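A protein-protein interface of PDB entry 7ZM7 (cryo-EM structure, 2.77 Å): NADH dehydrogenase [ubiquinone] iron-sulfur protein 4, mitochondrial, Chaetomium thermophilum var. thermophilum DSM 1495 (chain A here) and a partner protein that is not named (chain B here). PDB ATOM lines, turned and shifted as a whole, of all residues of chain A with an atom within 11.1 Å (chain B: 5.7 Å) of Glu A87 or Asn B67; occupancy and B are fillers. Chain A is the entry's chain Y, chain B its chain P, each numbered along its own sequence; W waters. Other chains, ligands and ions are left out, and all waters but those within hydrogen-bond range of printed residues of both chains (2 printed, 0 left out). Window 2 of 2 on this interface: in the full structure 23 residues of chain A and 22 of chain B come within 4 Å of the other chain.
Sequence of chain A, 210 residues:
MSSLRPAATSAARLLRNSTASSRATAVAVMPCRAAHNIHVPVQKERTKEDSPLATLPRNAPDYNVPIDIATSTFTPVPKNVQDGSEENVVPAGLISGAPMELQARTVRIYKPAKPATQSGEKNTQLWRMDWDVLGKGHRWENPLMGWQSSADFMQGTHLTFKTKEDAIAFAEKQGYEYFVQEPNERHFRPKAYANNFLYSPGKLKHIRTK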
ATOM      1  N   GLN A  82      23.575  -7.887  -6.742  1.00  0.00           N
ATOM      2  CA  GLN A  82      22.809  -9.064  -6.378  1.00  0.00           C
ATOM      3  C   GLN A  82      22.610  -9.948  -7.592  1.00  0.00           C
ATOM      4  O   GLN A  82      21.926  -9.577  -8.546  1.00  0.00           O
ATOM      5  CB  GLN A  82      21.458  -8.679  -5.790  1.00  0.00           C
ATOM      6  CG  GLN A  82      21.437  -8.486  -4.295  1.00  0.00           C
ATOM      7  CD  GLN A  82      20.084  -8.059  -3.813  1.00  0.00           C
ATOM      8  OE1 GLN A  82      19.316  -7.501  -4.570  1.00  0.00           O
ATOM      9  NE2 GLN A  82      19.786  -8.312  -2.553  1.00  0.00           N
ATOM     10  N   ASP A  83      23.231 -11.120  -7.548  1.00  0.00           N
ATOM     11  CA  ASP A  83      23.130 -12.116  -8.601  1.00  0.00           C
ATOM     12  C   ASP A  83      21.762 -12.769  -8.631  1.00  0.00           C
ATOM     13  O   ASP A  83      21.301 -13.191  -9.692  1.00  0.00           O
ATOM     14  CB  ASP A  83      24.207 -13.185  -8.392  1.00  0.00           C
ATOM     15  CG  ASP A  83      24.714 -13.769  -9.687  1.00  0.00           C
ATOM     16  OD1 ASP A  83      24.336 -13.258 -10.759  1.00  0.00           O
ATOM     17  OD2 ASP A  83      25.501 -14.735  -9.634  1.00  0.00           O
ATOM     18  N   GLY A  84      21.083 -12.820  -7.499  1.00  0.00           N
ATOM     19  CA  GLY A  84      19.828 -13.514  -7.407  1.00  0.00           C
ATOM     20  C   GLY A  84      19.959 -14.918  -6.918  1.00  0.00           C
ATOM     21  O   GLY A  84      19.053 -15.718  -7.143  1.00  0.00           O
ATOM     22  N   SER A  85      21.071 -15.246  -6.278  1.00  0.00           N
ATOM     23  CA  SER A  85      21.378 -16.585  -5.832  1.00  0.00           C
ATOM     24  C   SER A  85      21.652 -16.671  -4.346  1.00  0.00           C
ATOM     25  O   SER A  85      21.581 -17.771  -3.790  1.00  0.00           O
ATOM     26  CB  SER A  85      22.596 -17.113  -6.594  1.00  0.00           C
ATOM     27  OG  SER A  85      23.676 -16.212  -6.454  1.00  0.00           O
ATOM     28  N   GLU A  86      21.937 -15.550  -3.692  1.00  0.00           N
ATOM     29  CA  GLU A  86      22.348 -15.560  -2.300  1.00  0.00           C
ATOM     30  C   GLU A  86      21.274 -16.197  -1.433  1.00  0.00           C
ATOM     31  O   GLU A  86      20.077 -16.052  -1.687  1.00  0.00           O
ATOM     32  CB  GLU A  86      22.633 -14.130  -1.841  1.00  0.00           C
ATOM     33  CG  GLU A  86      23.181 -14.006  -0.431  1.00  0.00           C
ATOM     34  CD  GLU A  86      23.520 -12.573  -0.071  1.00  0.00           C
ATOM     35  OE1 GLU A  86      23.850 -12.311   1.104  1.00  0.00           O
ATOM     36  OE2 GLU A  86      23.456 -11.705  -0.966  1.00  0.00           O
ATOM     37  N   GLU A  87      21.707 -16.921  -0.411  1.00  0.00           N
ATOM     38  CA  GLU A  87      20.783 -17.714   0.383  1.00  0.00           C
ATOM     39  C   GLU A  87      20.030 -16.854   1.387  1.00  0.00           C
ATOM     40  O   GLU A  87      20.585 -15.922   1.972  1.00  0.00           O
ATOM     41  CB  GLU A  87      21.534 -18.830   1.102  1.00  0.00           C
ATOM     42  CG  GLU A  87      22.264 -19.757   0.149  1.00  0.00           C
ATOM     43  CD  GLU A  87      21.346 -20.356  -0.900  1.00  0.00           C
ATOM     44  OE1 GLU A  87      20.195 -20.707  -0.561  1.00  0.00           O
ATOM     45  OE2 GLU A  87      21.772 -20.469  -2.069  1.00  0.00           O
ATOM     46  N   ASN A  88      18.752 -17.176   1.565  1.00  0.00           N
ATOM     47  CA  ASN A  88      17.840 -16.687   2.591  1.00  0.00           C
ATOM     48  C   ASN A  88      17.383 -15.250   2.383  1.00  0.00           C
ATOM     49  O   ASN A  88      16.580 -14.766   3.180  1.00  0.00           O
ATOM     50  CB  ASN A  88      18.436 -16.802   4.002  1.00  0.00           C
ATOM     51  CG  ASN A  88      18.676 -18.235   4.413  1.00  0.00           C
ATOM     52  OD1 ASN A  88      18.058 -19.156   3.882  1.00  0.00           O
ATOM     53  ND2 ASN A  88      19.580 -18.433   5.363  1.00  0.00           N
ATOM     54  N   VAL A  89      17.847 -14.552   1.356  1.00  0.00           N
ATOM     55  CA  VAL A  89      17.460 -13.168   1.134  1.00  0.00           C
ATOM     56  C   VAL A  89      16.816 -13.068  -0.238  1.00  0.00           C
ATOM     57  O   VAL A  89      17.289 -13.680  -1.199  1.00  0.00           O
ATOM     58  CB  VAL A  89      18.660 -12.206   1.273  1.00  0.00           C
ATOM     59  CG1 VAL A  89      19.694 -12.445   0.197  1.00  0.00           C
ATOM     60  CG2 VAL A  89      18.199 -10.772   1.261  1.00  0.00           C
ATOM     61  N   VAL A  90      15.728 -12.324  -0.320  1.00  0.00           N
ATOM     62  CA  VAL A  90      15.137 -12.030  -1.628  1.00  0.00           C
ATOM     63  C   VAL A  90      16.051 -11.082  -2.385  1.00  0.00           C
ATOM     64  O   VAL A  90      16.528 -10.096  -1.803  1.00  0.00           O
ATOM     65  CB  VAL A  90      13.750 -11.425  -1.462  1.00  0.00           C
ATOM     66  CG1 VAL A  90      13.201 -11.030  -2.805  1.00  0.00           C
ATOM     67  CG2 VAL A  90      12.844 -12.399  -0.805  1.00  0.00           C
ATOM     68  N   PRO A  91      16.335 -11.327  -3.649  1.00  0.00           N
ATOM     69  CA  PRO A  91      17.105 -10.365  -4.449  1.00  0.00           C
ATOM     70  C   PRO A  91      16.235  -9.217  -4.953  1.00  0.00           C
ATOM     71  O   PRO A  91      15.994  -9.060  -6.141  1.00  0.00           O
ATOM     72  CB  PRO A  91      17.636 -11.250  -5.580  1.00  0.00           C
ATOM     73  CG  PRO A  91      16.572 -12.234  -5.774  1.00  0.00           C
ATOM     74  CD  PRO A  91      16.031 -12.542  -4.418  1.00  0.00           C
ATOM     75  N   ALA A  92      15.726  -8.414  -4.017  1.00  0.00           N
ATOM     76  CA  ALA A  92      14.773  -7.370  -4.375  1.00  0.00           C
ATOM     77  C   ALA A  92      15.420  -6.281  -5.214  1.00  0.00           C
ATOM     78  O   ALA A  92      14.760  -5.686  -6.066  1.00  0.00           O
ATOM     79  CB  ALA A  92      14.149  -6.768  -3.123  1.00  0.00           C
ATOM     80  N   LEU A  94      17.492  -6.792  -7.515  1.00  0.00           N
ATOM     81  CA  LEU A  94      17.530  -7.347  -8.858  1.00  0.00           C
ATOM     82  C   LEU A  94      16.224  -7.160  -9.615  1.00  0.00           C
ATOM     83  O   LEU A  94      16.244  -6.964 -10.830  1.00  0.00           O
ATOM     84  CB  LEU A  94      17.881  -8.829  -8.761  1.00  0.00           C
ATOM     85  CG  LEU A  94      17.708  -9.799  -9.916  1.00  0.00           C
ATOM     86  CD1 LEU A  94      18.699  -9.558 -11.037  1.00  0.00           C
ATOM     87  CD2 LEU A  94      17.832 -11.188  -9.357  1.00  0.00           C
ATOM     88  N   ILE A  95      15.093  -7.193  -8.925  1.00  0.00           N
ATOM     89  CA  ILE A  95      13.781  -7.090  -9.543  1.00  0.00           C
ATOM     90  C   ILE A  95      13.079  -5.780  -9.230  1.00  0.00           C
ATOM     91  O   ILE A  95      11.909  -5.623  -9.581  1.00  0.00           O
ATOM     92  CB  ILE A  95      12.894  -8.279  -9.135  1.00  0.00           C
ATOM     93  CG1 ILE A  95      12.969  -8.450  -7.620  1.00  0.00           C
ATOM     94  CG2 ILE A  95      13.309  -9.519  -9.881  1.00  0.00           C
ATOM     95  CD1 ILE A  95      12.008  -9.404  -7.055  1.00  0.00           C
ATOM     96  N   ALA A 169      17.320  -5.976   7.536  1.00  0.00           N
ATOM     97  CA  ALA A 169      16.619  -6.866   6.628  1.00  0.00           C
ATOM     98  C   ALA A 169      16.270  -6.162   5.322  1.00  0.00           C
ATOM     99  O   ALA A 169      16.431  -6.732   4.241  1.00  0.00           O
ATOM    100  CB  ALA A 169      15.374  -7.404   7.313  1.00  0.00           C
ATOM    101  N   GLU A 172      19.598  -5.554   3.202  1.00  0.00           N
ATOM    102  CA  GLU A 172      20.088  -6.735   2.515  1.00  0.00           C
ATOM    103  C   GLU A 172      19.137  -7.176   1.424  1.00  0.00           C
ATOM    104  O   GLU A 172      19.571  -7.716   0.407  1.00  0.00           O
ATOM    105  CB  GLU A 172      20.327  -7.864   3.501  1.00  0.00           C
ATOM    106  CG  GLU A 172      21.332  -7.519   4.565  1.00  0.00           C
ATOM    107  CD  GLU A 172      21.545  -8.644   5.556  1.00  0.00           C
ATOM    108  OE1 GLU A 172      22.011  -9.722   5.134  1.00  0.00           O
ATOM    109  OE2 GLU A 172      21.240  -8.466   6.749  1.00  0.00           O
ATOM    110  N   LYS A 173      17.842  -6.945   1.617  1.00  0.00           N
ATOM    111  CA  LYS A 173      16.860  -7.271   0.597  1.00  0.00           C
ATOM    112  C   LYS A 173      17.072  -6.435  -0.656  1.00  0.00           C
ATOM    113  O   LYS A 173      16.869  -6.929  -1.763  1.00  0.00           O
ATOM    114  CB  LYS A 173      15.460  -7.082   1.175  1.00  0.00           C
ATOM    115  CG  LYS A 173      14.321  -7.629   0.351  1.00  0.00           C
ATOM    116  CD  LYS A 173      13.002  -7.567   1.109  1.00  0.00           C
ATOM    117  CE  LYS A 173      12.738  -6.154   1.614  1.00  0.00           C
ATOM    118  NZ  LYS A 173      11.356  -5.953   2.102  1.00  0.00           N
ATOM    119  N   TRP B  18      10.239 -26.141 -11.393  1.00  0.00           N
ATOM    120  CA  TRP B  18      11.401 -25.697 -12.213  1.00  0.00           C
ATOM    121  C   TRP B  18      11.330 -26.216 -13.645  1.00  0.00           C
ATOM    122  O   TRP B  18      11.818 -25.502 -14.532  1.00  0.00           O
ATOM    123  CB  TRP B  18      12.731 -26.031 -11.531  1.00  0.00           C
ATOM    124  CG  TRP B  18      13.054 -25.095 -10.412  1.00  0.00           C
ATOM    125  CD1 TRP B  18      12.867 -25.305  -9.077  1.00  0.00           C
ATOM    126  CD2 TRP B  18      13.600 -23.772 -10.537  1.00  0.00           C
ATOM    127  NE1 TRP B  18      13.271 -24.211  -8.362  1.00  0.00           N
ATOM    128  CE2 TRP B  18      13.726 -23.254  -9.232  1.00  0.00           C
ATOM    129  CE3 TRP B  18      13.998 -22.980 -11.620  1.00  0.00           C
ATOM    130  CZ2 TRP B  18      14.234 -21.983  -8.986  1.00  0.00           C
ATOM    131  CZ3 TRP B  18      14.498 -21.722 -11.375  1.00  0.00           C
ATOM    132  CH2 TRP B  18      14.615 -21.234 -10.074  1.00  0.00           C
ATOM    133  N   TYR B  65      21.405 -16.984 -12.958  1.00  0.00           N
ATOM    134  CA  TYR B  65      21.738 -17.650 -11.715  1.00  0.00           C
ATOM    135  C   TYR B  65      20.663 -17.514 -10.651  1.00  0.00           C
ATOM    136  O   TYR B  65      20.960 -17.682  -9.469  1.00  0.00           O
ATOM    137  CB  TYR B  65      23.053 -17.091 -11.192  1.00  0.00           C
ATOM    138  CG  TYR B  65      24.090 -17.042 -12.259  1.00  0.00           C
ATOM    139  CD1 TYR B  65      24.727 -18.192 -12.672  1.00  0.00           C
ATOM    140  CD2 TYR B  65      24.412 -15.855 -12.886  1.00  0.00           C
ATOM    141  CE1 TYR B  65      25.662 -18.164 -13.649  1.00  0.00           C
ATOM    142  CE2 TYR B  65      25.360 -15.816 -13.876  1.00  0.00           C
ATOM    143  CZ  TYR B  65      25.982 -16.980 -14.253  1.00  0.00           C
ATOM    144  OH  TYR B  65      26.935 -16.954 -15.246  1.00  0.00           O
ATOM    145  N   VAL B  66      19.457 -17.117 -11.058  1.00  0.00           N
ATOM    146  CA  VAL B  66      18.361 -17.055 -10.056  1.00  0.00           C
ATOM    147  C   VAL B  66      17.881 -18.458  -9.697  1.00  0.00           C
ATOM    148  O   VAL B  66      17.431 -19.178 -10.595  1.00  0.00           O
ATOM    149  CB  VAL B  66      17.216 -16.143 -10.532  1.00  0.00           C
ATOM    150  CG1 VAL B  66      16.047 -16.170  -9.564  1.00  0.00           C
ATOM    151  CG2 VAL B  66      17.692 -14.719 -10.764  1.00  0.00           C
ATOM    152  N   ASN B  67      17.975 -18.811  -8.416  1.00  0.00           N
ATOM    153  CA  ASN B  67      17.549 -20.117  -7.940  1.00  0.00           C
ATOM    154  C   ASN B  67      16.315 -20.037  -7.061  1.00  0.00           C
ATOM    155  O   ASN B  67      16.095 -20.911  -6.225  1.00  0.00           O
ATOM    156  CB  ASN B  67      18.679 -20.797  -7.179  1.00  0.00           C
ATOM    157  CG  ASN B  67      19.024 -20.080  -5.918  1.00  0.00           C
ATOM    158  OD1 ASN B  67      19.219 -18.876  -5.916  1.00  0.00           O
ATOM    159  ND2 ASN B  67      19.069 -20.811  -4.819  1.00  0.00           N
ATOM    160  N   LYS B  68      15.522 -18.995  -7.219  1.00  0.00           N
ATOM    161  CA  LYS B  68      14.249 -18.840  -6.538  1.00  0.00           C
ATOM    162  C   LYS B  68      13.132 -18.873  -7.557  1.00  0.00           C
ATOM    163  O   LYS B  68      13.200 -18.188  -8.576  1.00  0.00           O
ATOM    164  CB  LYS B  68      14.200 -17.544  -5.751  1.00  0.00           C
ATOM    165  CG  LYS B  68      14.833 -17.633  -4.404  1.00  0.00           C
ATOM    166  CD  LYS B  68      16.313 -17.692  -4.395  1.00  0.00           C
ATOM    167  CE  LYS B  68      16.920 -16.417  -4.812  1.00  0.00           C
ATOM    168  NZ  LYS B  68      18.365 -16.583  -4.696  1.00  0.00           N
ATOM    169  N   LEU B  69      12.124 -19.691  -7.294  1.00  0.00           N
ATOM    170  CA  LEU B  69      11.014 -19.809  -8.223  1.00  0.00           C
ATOM    171  C   LEU B  69      10.076 -18.613  -8.152  1.00  0.00           C
ATOM    172  O   LEU B  69       9.454 -18.263  -9.156  1.00  0.00           O
ATOM    173  CB  LEU B  69      10.256 -21.109  -7.958  1.00  0.00           C
ATOM    174  CG  LEU B  69       9.630 -21.765  -9.188  1.00  0.00           C
ATOM    175  CD1 LEU B  69      10.639 -21.771 -10.279  1.00  0.00           C
ATOM    176  CD2 LEU B  69       9.171 -23.167  -8.894  1.00  0.00           C
HETATM  177  O   HOH W   1      21.820 -14.091 -12.181  1.00  0.00           O
HETATM  178  O   HOH W   2      19.422 -13.677  -3.327  1.00  0.00           O
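NZ of Lys B68 is in hydrogen-bond range of O of Gly A84.
The side-chain amide oxygen of Asn B67 sits close to the backbone carbonyl oxygen of Gly A84, 3.4 Å away.
The backbone carbonyl oxygen (O) of Ser A85 sits close to the side-chain amide oxygen (OD1) of Asn B67.
The backbone NH (N) of Ser A85 sits close to the side-chain amino group (NZ) of Lys B68 (3.4 Å).
The side-chain amide oxygen (OD1) of Asn B67 is in hydrogen-bond range of the side-chain amino group (NZ) of Lys B68 (2.7 Å).
Among the printed residues, pairs that only touch across the chains: Asp A83 with Tyr B65, Gly A84 with Tyr B65, Gly A84 with Val B66, Ser A85 with Tyr B65, Glu A86 with Lys B68, Glu A87 with Asn B67, Pro A91 with Lys B68 and Leu A94 with Val B66.
Gln A82 touches none of the printed residues of chain B.
Printed residues of chain B within 4 Å of Glu A86: Lys B68 (3.5 Å).
Of chain B, only Asn B67 comes within 4 Å of Glu A87.
Of chain A, only Gly A84 (3.4 Å), Ser A85 (3.1 Å) and Glu A87 (3.9 Å) come within 4 Å of Asn B67.
Printed residues of chain A within 4 Å of Lys B68: Gly A84 (2.7 Å), Ser A85 (3.2 Å), Glu A86 (3.5 Å) and Pro A91 (3.995 Å).
The nearest residue of chain A that does not touch Asn B67 is Glu A86 (4.8 Å).
Hydrophobic or aromatic side chains of chain A within 4 Å of the printed part of chain B: Pro A91 and Leu A94.
Of the 6 printed residues of chain B, 4 touch a printed residue of chain A.
Hydrophobic or aromatic side chains of chain B that line the printed part of chain A: Tyr B65 and Val B66.
Among the printed residues, 12 pairs touch across the chains.
Among the printed residues, no Asp or Glu carboxylate lies within 4 Å of a Lys or Arg side-chain nitrogen of the other chain.
Water W1 lies within hydrogen-bond range of the backbone carbonyl oxygen of Asp A83 (2.7 Å) and the backbone NH of Tyr B65 (3.0 Å).
Water W2 lies within hydrogen-bond range of O of Glu A86 (3.0 Å), O of Val A89 (3.0 Å) and NZ of Lys B68 (3.4 Å).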
